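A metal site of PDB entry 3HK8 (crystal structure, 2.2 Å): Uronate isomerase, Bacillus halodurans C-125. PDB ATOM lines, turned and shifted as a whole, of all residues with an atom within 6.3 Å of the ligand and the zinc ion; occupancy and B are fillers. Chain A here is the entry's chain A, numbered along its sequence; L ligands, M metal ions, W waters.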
ATOM      1  N   HIS A  26     -16.306   1.285  -2.389  1.00  0.00           N
ATOM      2  CA  HIS A  26     -17.751   1.297  -2.229  1.00  0.00           C
ATOM      3  C   HIS A  26     -18.177   1.990  -0.945  1.00  0.00           C
ATOM      4  O   HIS A  26     -17.939   1.487   0.154  1.00  0.00           O
ATOM      5  CB  HIS A  26     -18.375  -0.100  -2.249  1.00  0.00           C
ATOM      6  CG  HIS A  26     -19.854  -0.087  -1.990  1.00  0.00           C
ATOM      7  ND1 HIS A  26     -20.734   0.660  -2.745  1.00  0.00           N
ATOM      8  CD2 HIS A  26     -20.594  -0.679  -1.024  1.00  0.00           C
ATOM      9  CE1 HIS A  26     -21.952   0.532  -2.256  1.00  0.00           C
ATOM     10  NE2 HIS A  26     -21.893  -0.277  -1.214  1.00  0.00           N
ATOM     11  N   THR A  27     -18.806   3.147  -1.106  1.00  0.00           N
ATOM     12  CA  THR A  27     -19.301   3.934   0.020  1.00  0.00           C
ATOM     13  C   THR A  27     -20.612   4.588  -0.388  1.00  0.00           C
ATOM     14  O   THR A  27     -21.057   4.460  -1.538  1.00  0.00           O
ATOM     15  CB  THR A  27     -18.344   5.079   0.414  1.00  0.00           C
ATOM     16  OG1 THR A  27     -18.472   6.143  -0.542  1.00  0.00           O
ATOM     17  CG2 THR A  27     -16.888   4.596   0.445  1.00  0.00           C
ATOM     18  N   HIS A  28     -21.214   5.289   0.556  1.00  0.00           N
ATOM     19  CA  HIS A  28     -22.452   6.016   0.331  1.00  0.00           C
ATOM     20  C   HIS A  28     -22.167   7.458   0.722  1.00  0.00           C
ATOM     21  O   HIS A  28     -23.013   8.157   1.300  1.00  0.00           O
ATOM     22  CB  HIS A  28     -23.577   5.409   1.182  1.00  0.00           C
ATOM     23  CG  HIS A  28     -23.933   4.018   0.778  1.00  0.00           C
ATOM     24  ND1 HIS A  28     -24.807   3.748  -0.252  1.00  0.00           N
ATOM     25  CD2 HIS A  28     -23.479   2.823   1.209  1.00  0.00           C
ATOM     26  CE1 HIS A  28     -24.869   2.444  -0.447  1.00  0.00           C
ATOM     27  NE2 HIS A  28     -24.068   1.856   0.430  1.00  0.00           N
ATOM     28  N   TYR A  48     -26.801   6.402  12.687  1.00  0.00           N
ATOM     29  CA  TYR A  48     -26.481   5.443  11.612  1.00  0.00           C
ATOM     30  C   TYR A  48     -27.529   4.336  11.778  1.00  0.00           C
ATOM     31  O   TYR A  48     -27.824   3.941  12.907  1.00  0.00           O
ATOM     32  CB  TYR A  48     -25.063   4.928  11.866  1.00  0.00           C
ATOM     33  CG  TYR A  48     -24.505   3.896  10.918  1.00  0.00           C
ATOM     34  CD1 TYR A  48     -24.731   3.962   9.543  1.00  0.00           C
ATOM     35  CD2 TYR A  48     -23.626   2.907  11.397  1.00  0.00           C
ATOM     36  CE1 TYR A  48     -24.090   3.076   8.663  1.00  0.00           C
ATOM     37  CE2 TYR A  48     -22.986   2.025  10.534  1.00  0.00           C
ATOM     38  CZ  TYR A  48     -23.220   2.111   9.161  1.00  0.00           C
ATOM     39  OH  TYR A  48     -22.559   1.250   8.312  1.00  0.00           O
ATOM     40  N   HIS A  49     -28.090   3.808  10.698  1.00  0.00           N
ATOM     41  CA  HIS A  49     -29.134   2.798  10.868  1.00  0.00           C
ATOM     42  C   HIS A  49     -28.710   1.540  11.612  1.00  0.00           C
ATOM     43  O   HIS A  49     -29.556   0.868  12.218  1.00  0.00           O
ATOM     44  CB  HIS A  49     -29.841   2.469   9.534  1.00  0.00           C
ATOM     45  CG  HIS A  49     -29.067   1.562   8.623  1.00  0.00           C
ATOM     46  ND1 HIS A  49     -29.044   0.192   8.775  1.00  0.00           N
ATOM     47  CD2 HIS A  49     -28.346   1.827   7.511  1.00  0.00           C
ATOM     48  CE1 HIS A  49     -28.341  -0.345   7.797  1.00  0.00           C
ATOM     49  NE2 HIS A  49     -27.903   0.622   7.006  1.00  0.00           N
ATOM     50  N   TYR A  50     -27.423   1.230  11.623  1.00  0.00           N
ATOM     51  CA  TYR A  50     -26.944   0.060  12.357  1.00  0.00           C
ATOM     52  C   TYR A  50     -27.256   0.257  13.842  1.00  0.00           C
ATOM     53  O   TYR A  50     -27.553  -0.705  14.545  1.00  0.00           O
ATOM     54  CB  TYR A  50     -25.419  -0.129  12.202  1.00  0.00           C
ATOM     55  CG  TYR A  50     -24.950  -0.679  10.867  1.00  0.00           C
ATOM     56  CD1 TYR A  50     -25.519  -0.244   9.672  1.00  0.00           C
ATOM     57  CD2 TYR A  50     -23.871  -1.567  10.804  1.00  0.00           C
ATOM     58  CE1 TYR A  50     -25.031  -0.689   8.441  1.00  0.00           C
ATOM     59  CE2 TYR A  50     -23.371  -2.016   9.575  1.00  0.00           C
ATOM     60  CZ  TYR A  50     -23.959  -1.566   8.399  1.00  0.00           C
ATOM     61  OH  TYR A  50     -23.455  -1.962   7.176  1.00  0.00           O
ATOM     62  N   THR A 143     -21.830   5.979  -4.499  1.00  0.00           N
ATOM     63  CA  THR A 143     -22.915   5.136  -4.991  1.00  0.00           C
ATOM     64  C   THR A 143     -23.857   6.213  -5.562  1.00  0.00           C
ATOM     65  O   THR A 143     -24.467   6.974  -4.808  1.00  0.00           O
ATOM     66  CB  THR A 143     -23.652   4.374  -3.866  1.00  0.00           C
ATOM     67  OG1 THR A 143     -22.775   3.384  -3.315  1.00  0.00           O
ATOM     68  CG2 THR A 143     -24.890   3.675  -4.423  1.00  0.00           C
ATOM     69  N   ARG A 170     -25.314   3.186  -9.830  1.00  0.00           N
ATOM     70  CA  ARG A 170     -26.168   2.234  -9.125  1.00  0.00           C
ATOM     71  C   ARG A 170     -27.452   2.053  -9.933  1.00  0.00           C
ATOM     72  O   ARG A 170     -28.104   3.038 -10.301  1.00  0.00           O
ATOM     73  CB  ARG A 170     -26.486   2.744  -7.717  1.00  0.00           C
ATOM     74  CG  ARG A 170     -27.400   1.802  -6.917  1.00  0.00           C
ATOM     75  CD  ARG A 170     -26.797   0.406  -6.757  1.00  0.00           C
ATOM     76  NE  ARG A 170     -25.864   0.344  -5.644  1.00  0.00           N
ATOM     77  CZ  ARG A 170     -26.131  -0.211  -4.463  1.00  0.00           C
ATOM     78  NH1 ARG A 170     -27.300  -0.785  -4.212  1.00  0.00           N
ATOM     79  NH2 ARG A 170     -25.221  -0.153  -3.495  1.00  0.00           N
ATOM     80  N   ASP A 172     -30.255  -0.385  -9.068  1.00  0.00           N
ATOM     81  CA  ASP A 172     -31.327  -1.142  -8.414  1.00  0.00           C
ATOM     82  C   ASP A 172     -32.748  -0.902  -8.960  1.00  0.00           C
ATOM     83  O   ASP A 172     -33.456  -1.859  -9.287  1.00  0.00           O
ATOM     84  CB  ASP A 172     -31.304  -0.890  -6.902  1.00  0.00           C
ATOM     85  CG  ASP A 172     -30.064  -1.462  -6.225  1.00  0.00           C
ATOM     86  OD1 ASP A 172     -29.056  -1.693  -6.933  1.00  0.00           O
ATOM     87  OD2 ASP A 172     -30.087  -1.682  -5.001  1.00  0.00           O
ATOM     88  N   SER A 223     -27.706  -4.245  -6.076  1.00  0.00           N
ATOM     89  CA  SER A 223     -27.785  -5.153  -4.944  1.00  0.00           C
ATOM     90  C   SER A 223     -28.890  -6.130  -5.367  1.00  0.00           C
ATOM     91  O   SER A 223     -29.906  -5.717  -5.930  1.00  0.00           O
ATOM     92  CB  SER A 223     -28.148  -4.423  -3.641  1.00  0.00           C
ATOM     93  OG  SER A 223     -29.425  -3.826  -3.687  1.00  0.00           O
ATOM     94  N   MET A 258     -23.963  -7.090  -5.549  1.00  0.00           N
ATOM     95  CA  MET A 258     -23.961  -7.228  -4.098  1.00  0.00           C
ATOM     96  C   MET A 258     -25.169  -8.132  -3.822  1.00  0.00           C
ATOM     97  O   MET A 258     -26.317  -7.670  -3.775  1.00  0.00           O
ATOM     98  CB  MET A 258     -24.108  -5.846  -3.444  1.00  0.00           C
ATOM     99  CG  MET A 258     -23.075  -4.819  -3.973  1.00  0.00           C
ATOM    100  SD  MET A 258     -22.941  -3.249  -3.067  1.00  0.00           S
ATOM    101  CE  MET A 258     -21.692  -3.714  -1.893  1.00  0.00           C
ATOM    102  N   VAL A 261     -29.265  -9.703  -0.175  1.00  0.00           N
ATOM    103  CA  VAL A 261     -30.108  -8.846   0.661  1.00  0.00           C
ATOM    104  C   VAL A 261     -31.615  -9.029   0.433  1.00  0.00           C
ATOM    105  O   VAL A 261     -32.087  -8.973  -0.692  1.00  0.00           O
ATOM    106  CB  VAL A 261     -29.751  -7.343   0.458  1.00  0.00           C
ATOM    107  CG1 VAL A 261     -29.981  -6.935  -0.993  1.00  0.00           C
ATOM    108  CG2 VAL A 261     -30.575  -6.484   1.388  1.00  0.00           C
ATOM    109  N   LYS A 263     -34.836  -7.294   1.096  1.00  0.00           N
ATOM    110  CA  LYS A 263     -35.353  -5.977   1.427  1.00  0.00           C
ATOM    111  C   LYS A 263     -36.628  -5.917   2.258  1.00  0.00           C
ATOM    112  O   LYS A 263     -37.540  -6.731   2.111  1.00  0.00           O
ATOM    113  CB  LYS A 263     -35.592  -5.162   0.140  1.00  0.00           C
ATOM    114  CG  LYS A 263     -34.420  -5.140  -0.848  1.00  0.00           C
ATOM    115  CD  LYS A 263     -33.204  -4.416  -0.291  1.00  0.00           C
ATOM    116  CE  LYS A 263     -33.430  -2.916  -0.190  1.00  0.00           C
ATOM    117  NZ  LYS A 263     -32.238  -2.189   0.330  1.00  0.00           N
ATOM    118  N   ASP A 271     -34.184   1.985   6.635  1.00  0.00           N
ATOM    119  CA  ASP A 271     -32.919   1.418   6.178  1.00  0.00           C
ATOM    120  C   ASP A 271     -32.398   0.287   7.066  1.00  0.00           C
ATOM    121  O   ASP A 271     -31.575  -0.511   6.630  1.00  0.00           O
ATOM    122  CB  ASP A 271     -31.850   2.519   6.073  1.00  0.00           C
ATOM    123  CG  ASP A 271     -32.090   3.454   4.909  1.00  0.00           C
ATOM    124  OD1 ASP A 271     -32.692   3.021   3.896  1.00  0.00           O
ATOM    125  OD2 ASP A 271     -31.668   4.626   4.989  1.00  0.00           O
ATOM    126  N   ASP A 274     -33.629  -4.339   6.535  1.00  0.00           N
ATOM    127  CA  ASP A 274     -33.258  -5.387   5.587  1.00  0.00           C
ATOM    128  C   ASP A 274     -32.651  -6.621   6.263  1.00  0.00           C
ATOM    129  O   ASP A 274     -31.936  -6.509   7.265  1.00  0.00           O
ATOM    130  CB  ASP A 274     -32.290  -4.843   4.523  1.00  0.00           C
ATOM    131  CG  ASP A 274     -32.891  -3.727   3.700  1.00  0.00           C
ATOM    132  OD1 ASP A 274     -34.139  -3.710   3.556  1.00  0.00           O
ATOM    133  OD2 ASP A 274     -32.128  -2.872   3.195  1.00  0.00           O
ATOM    134  N   TRP A 325     -19.065  -7.299   3.466  1.00  0.00           N
ATOM    135  CA  TRP A 325     -20.254  -6.487   3.397  1.00  0.00           C
ATOM    136  C   TRP A 325     -21.337  -6.548   4.474  1.00  0.00           C
ATOM    137  O   TRP A 325     -21.845  -7.629   4.820  1.00  0.00           O
ATOM    138  CB  TRP A 325     -20.894  -6.746   2.028  1.00  0.00           C
ATOM    139  CG  TRP A 325     -22.104  -5.935   1.694  1.00  0.00           C
ATOM    140  CD1 TRP A 325     -22.295  -4.603   1.943  1.00  0.00           C
ATOM    141  CD2 TRP A 325     -23.255  -6.372   0.957  1.00  0.00           C
ATOM    142  NE1 TRP A 325     -23.502  -4.188   1.394  1.00  0.00           N
ATOM    143  CE2 TRP A 325     -24.106  -5.247   0.781  1.00  0.00           C
ATOM    144  CE3 TRP A 325     -23.652  -7.607   0.418  1.00  0.00           C
ATOM    145  CZ2 TRP A 325     -25.326  -5.331   0.104  1.00  0.00           C
ATOM    146  CZ3 TRP A 325     -24.861  -7.682  -0.260  1.00  0.00           C
ATOM    147  CH2 TRP A 325     -25.681  -6.548  -0.412  1.00  0.00           C
ATOM    148  N   TRP A 326     -21.671  -5.371   5.002  1.00  0.00           N
ATOM    149  CA  TRP A 326     -22.765  -5.190   5.953  1.00  0.00           C
ATOM    150  C   TRP A 326     -22.739  -6.113   7.175  1.00  0.00           C
ATOM    151  O   TRP A 326     -21.980  -5.895   8.122  1.00  0.00           O
ATOM    152  CB  TRP A 326     -24.051  -5.415   5.148  1.00  0.00           C
ATOM    153  CG  TRP A 326     -25.307  -4.755   5.621  1.00  0.00           C
ATOM    154  CD1 TRP A 326     -25.628  -4.342   6.884  1.00  0.00           C
ATOM    155  CD2 TRP A 326     -26.477  -4.536   4.814  1.00  0.00           C
ATOM    156  NE1 TRP A 326     -26.930  -3.893   6.920  1.00  0.00           N
ATOM    157  CE2 TRP A 326     -27.468  -4.001   5.661  1.00  0.00           C
ATOM    158  CE3 TRP A 326     -26.772  -4.755   3.464  1.00  0.00           C
ATOM    159  CZ2 TRP A 326     -28.753  -3.669   5.203  1.00  0.00           C
ATOM    160  CZ3 TRP A 326     -28.065  -4.425   3.000  1.00  0.00           C
ATOM    161  CH2 TRP A 326     -29.022  -3.894   3.873  1.00  0.00           C
ATOM    162  N   PHE A 327     -23.579  -7.142   7.164  1.00  0.00           N
ATOM    163  CA  PHE A 327     -23.647  -8.087   8.281  1.00  0.00           C
ATOM    164  C   PHE A 327     -22.381  -8.945   8.386  1.00  0.00           C
ATOM    165  O   PHE A 327     -22.195  -9.647   9.382  1.00  0.00           O
ATOM    166  CB  PHE A 327     -24.885  -8.983   8.141  1.00  0.00           C
ATOM    167  CG  PHE A 327     -26.178  -8.216   8.042  1.00  0.00           C
ATOM    168  CD1 PHE A 327     -26.516  -7.262   9.005  1.00  0.00           C
ATOM    169  CD2 PHE A 327     -27.042  -8.413   6.968  1.00  0.00           C
ATOM    170  CE1 PHE A 327     -27.699  -6.508   8.901  1.00  0.00           C
ATOM    171  CE2 PHE A 327     -28.227  -7.669   6.855  1.00  0.00           C
ATOM    172  CZ  PHE A 327     -28.553  -6.719   7.819  1.00  0.00           C
ATOM    173  N   HIS A 353     -13.977  -2.673   2.005  1.00  0.00           N
ATOM    174  CA  HIS A 353     -14.541  -1.413   1.556  1.00  0.00           C
ATOM    175  C   HIS A 353     -15.287  -0.960   2.821  1.00  0.00           C
ATOM    176  O   HIS A 353     -15.641  -1.789   3.646  1.00  0.00           O
ATOM    177  CB  HIS A 353     -15.504  -1.586   0.360  1.00  0.00           C
ATOM    178  CG  HIS A 353     -16.773  -2.306   0.691  1.00  0.00           C
ATOM    179  ND1 HIS A 353     -16.894  -3.688   0.626  1.00  0.00           N
ATOM    180  CD2 HIS A 353     -17.986  -1.845   1.089  1.00  0.00           C
ATOM    181  CE1 HIS A 353     -18.124  -4.027   0.963  1.00  0.00           C
ATOM    182  NE2 HIS A 353     -18.806  -2.930   1.249  1.00  0.00           N
ATOM    183  N   ASP A 355     -18.289   1.152   2.985  1.00  0.00           N
ATOM    184  CA  ASP A 355     -19.739   1.242   2.858  1.00  0.00           C
ATOM    185  C   ASP A 355     -20.212   2.404   3.736  1.00  0.00           C
ATOM    186  O   ASP A 355     -21.355   2.425   4.180  1.00  0.00           O
ATOM    187  CB  ASP A 355     -20.394  -0.058   3.324  1.00  0.00           C
ATOM    188  CG  ASP A 355     -21.451  -0.546   2.342  1.00  0.00           C
ATOM    189  OD1 ASP A 355     -22.295   0.262   1.913  1.00  0.00           O
ATOM    190  OD2 ASP A 355     -21.422  -1.746   2.012  1.00  0.00           O
ATOM    191  N   ARG A 357     -21.739   5.611   5.303  1.00  0.00           N
ATOM    192  CA  ARG A 357     -22.918   6.428   5.045  1.00  0.00           C
ATOM    193  C   ARG A 357     -22.698   7.804   5.658  1.00  0.00           C
ATOM    194  O   ARG A 357     -23.287   8.792   5.222  1.00  0.00           O
ATOM    195  CB  ARG A 357     -24.171   5.787   5.667  1.00  0.00           C
ATOM    196  CG  ARG A 357     -24.844   4.762   4.784  1.00  0.00           C
ATOM    197  CD  ARG A 357     -25.850   3.954   5.563  1.00  0.00           C
ATOM    198  NE  ARG A 357     -26.661   3.101   4.703  1.00  0.00           N
ATOM    199  CZ  ARG A 357     -27.709   3.521   3.990  1.00  0.00           C
ATOM    200  NH1 ARG A 357     -28.078   4.792   4.019  1.00  0.00           N
ATOM    201  NH2 ARG A 357     -28.389   2.651   3.258  1.00  0.00           N
HETATM  202  O1  LIG L   1     -25.072  -0.865  -0.965  1.00  0.00           O
HETATM  203  C1  LIG L   1     -26.008  -1.423  -0.339  1.00  0.00           C
HETATM  204  O2  LIG L   1     -27.068  -1.849  -0.856  1.00  0.00           O
HETATM  205  C2  LIG L   1     -25.858  -1.630   1.185  1.00  0.00           C
HETATM  206  O3  LIG L   1     -24.484  -1.456   1.544  1.00  0.00           O
HETATM  207  C3  LIG L   1     -26.771  -0.621   1.927  1.00  0.00           C
HETATM  208  O4  LIG L   1     -26.323   0.728   1.754  1.00  0.00           O
HETATM  209  C4  LIG L   1     -26.894  -0.859   3.486  1.00  0.00           C
HETATM  210  O5  LIG L   1     -28.078  -0.261   3.993  1.00  0.00           O
HETATM  211  C5  LIG L   1     -25.702  -0.303   4.307  1.00  0.00           C
HETATM  212  O6  LIG L   1     -25.847   0.566   5.166  1.00  0.00           O
HETATM  213  N1  LIG L   1     -24.483  -0.807   4.042  1.00  0.00           N
HETATM  214  O7  LIG L   1     -24.121  -2.066   4.417  1.00  0.00           O
HETATM  215 ZN    ZN M   1     -23.450  -0.089   0.273  1.00  0.00          ZN
HETATM  216  O   HOH W   1     -23.145   1.371   5.693  1.00  0.00           O
HETATM  217  O   HOH W   2     -29.586  -2.951  -0.859  1.00  0.00           O
HETATM  218  O   HOH W   3     -30.720  -0.876   4.344  1.00  0.00           O
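The zinc ion is bound by OD1 of Asp 355 (2.0 Å), NE2 of His 28 (2.0 Å), O3 of the ligand (2.1 Å), NE2 of His 26 (2.2 Å) and O1 of the ligand (2.2 Å). The zinc ion has five donor atoms within binding distance.
Water W3 lies within hydrogen-bond range of the backbone carbonyl oxygen of Asp 271, the side-chain carboxylate of Asp 274 and an oxygen (O5) of the ligand. Water W2 lies within hydrogen-bond range of O2 of the ligand (2.7 Å), OG of Ser 223 (3.0 Å) and NZ of Lys 263 (3.0 Å). Water W1 lies within hydrogen-bond range of the backbone carbonyl oxygen of Asp 355 (2.6 Å), the side-chain hydroxyl of Tyr 48 (2.7 Å) and an oxygen (O6) of the ligand (2.9 Å).
Ser 223 touches the ligand (CB to O2, 3.9 Å). SD of Met 258 touches O1 of the ligand (3.8 Å). Trp 326 touches the ligand (CG to O7, 3.2 Å). 11 residues have an atom within 4 Å of the ligand: His 26, His 28, His 49, Tyr 50, Arg 170, Ser 223, Met 258, Trp 325, Trp 326, Asp 355 and Arg 357. The nearest printed residue that does not touch the ligand is Asp 271 (4.4 Å).
A ring nitrogen (ND1) of His 26 lies close to the side-chain hydroxyl (OG1) of Thr 143. The guanidinium group (NH1) of Arg 357 lies within salt-bridge range of the side-chain carboxylate (OD2) of Asp 271 (3.7 Å). OD2 of Asp 172 is in hydrogen-bond range of OG of Ser 223 (2.6 Å). NE2 of His 26 lies close to SD of Met 258. OD2 of Asp 172 is in salt-bridge range of NH1 of Arg 170, 3.0 Å away. A ring nitrogen (ND1) of His 49 sits at hydrogen-bond distance from the backbone carbonyl oxygen (O) of Asp 271 (3.4 Å). The side-chain carboxylate (OD2) of Asp 355 sits at hydrogen-bond distance from a ring nitrogen (NE2) of His 353 (3.0 Å). OD2 of Asp 355 sits close to NE1 of Trp 325 (3.3 Å).
An oxygen (O6) of the ligand is in hydrogen-bond range of a ring nitrogen (NE2) of His 49, at 2.8 Å. O6 of the ligand is in hydrogen-bond range of NE of Arg 357, at 2.7 Å. OH of Tyr 50 is in hydrogen-bond range of O7 of the ligand (2.8 Å). NH1 of Arg 170 is in salt-bridge range of O2 of the ligand. An oxygen (O3) of the ligand lies close to the indole nitrogen of Trp 325 (2.9 Å).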
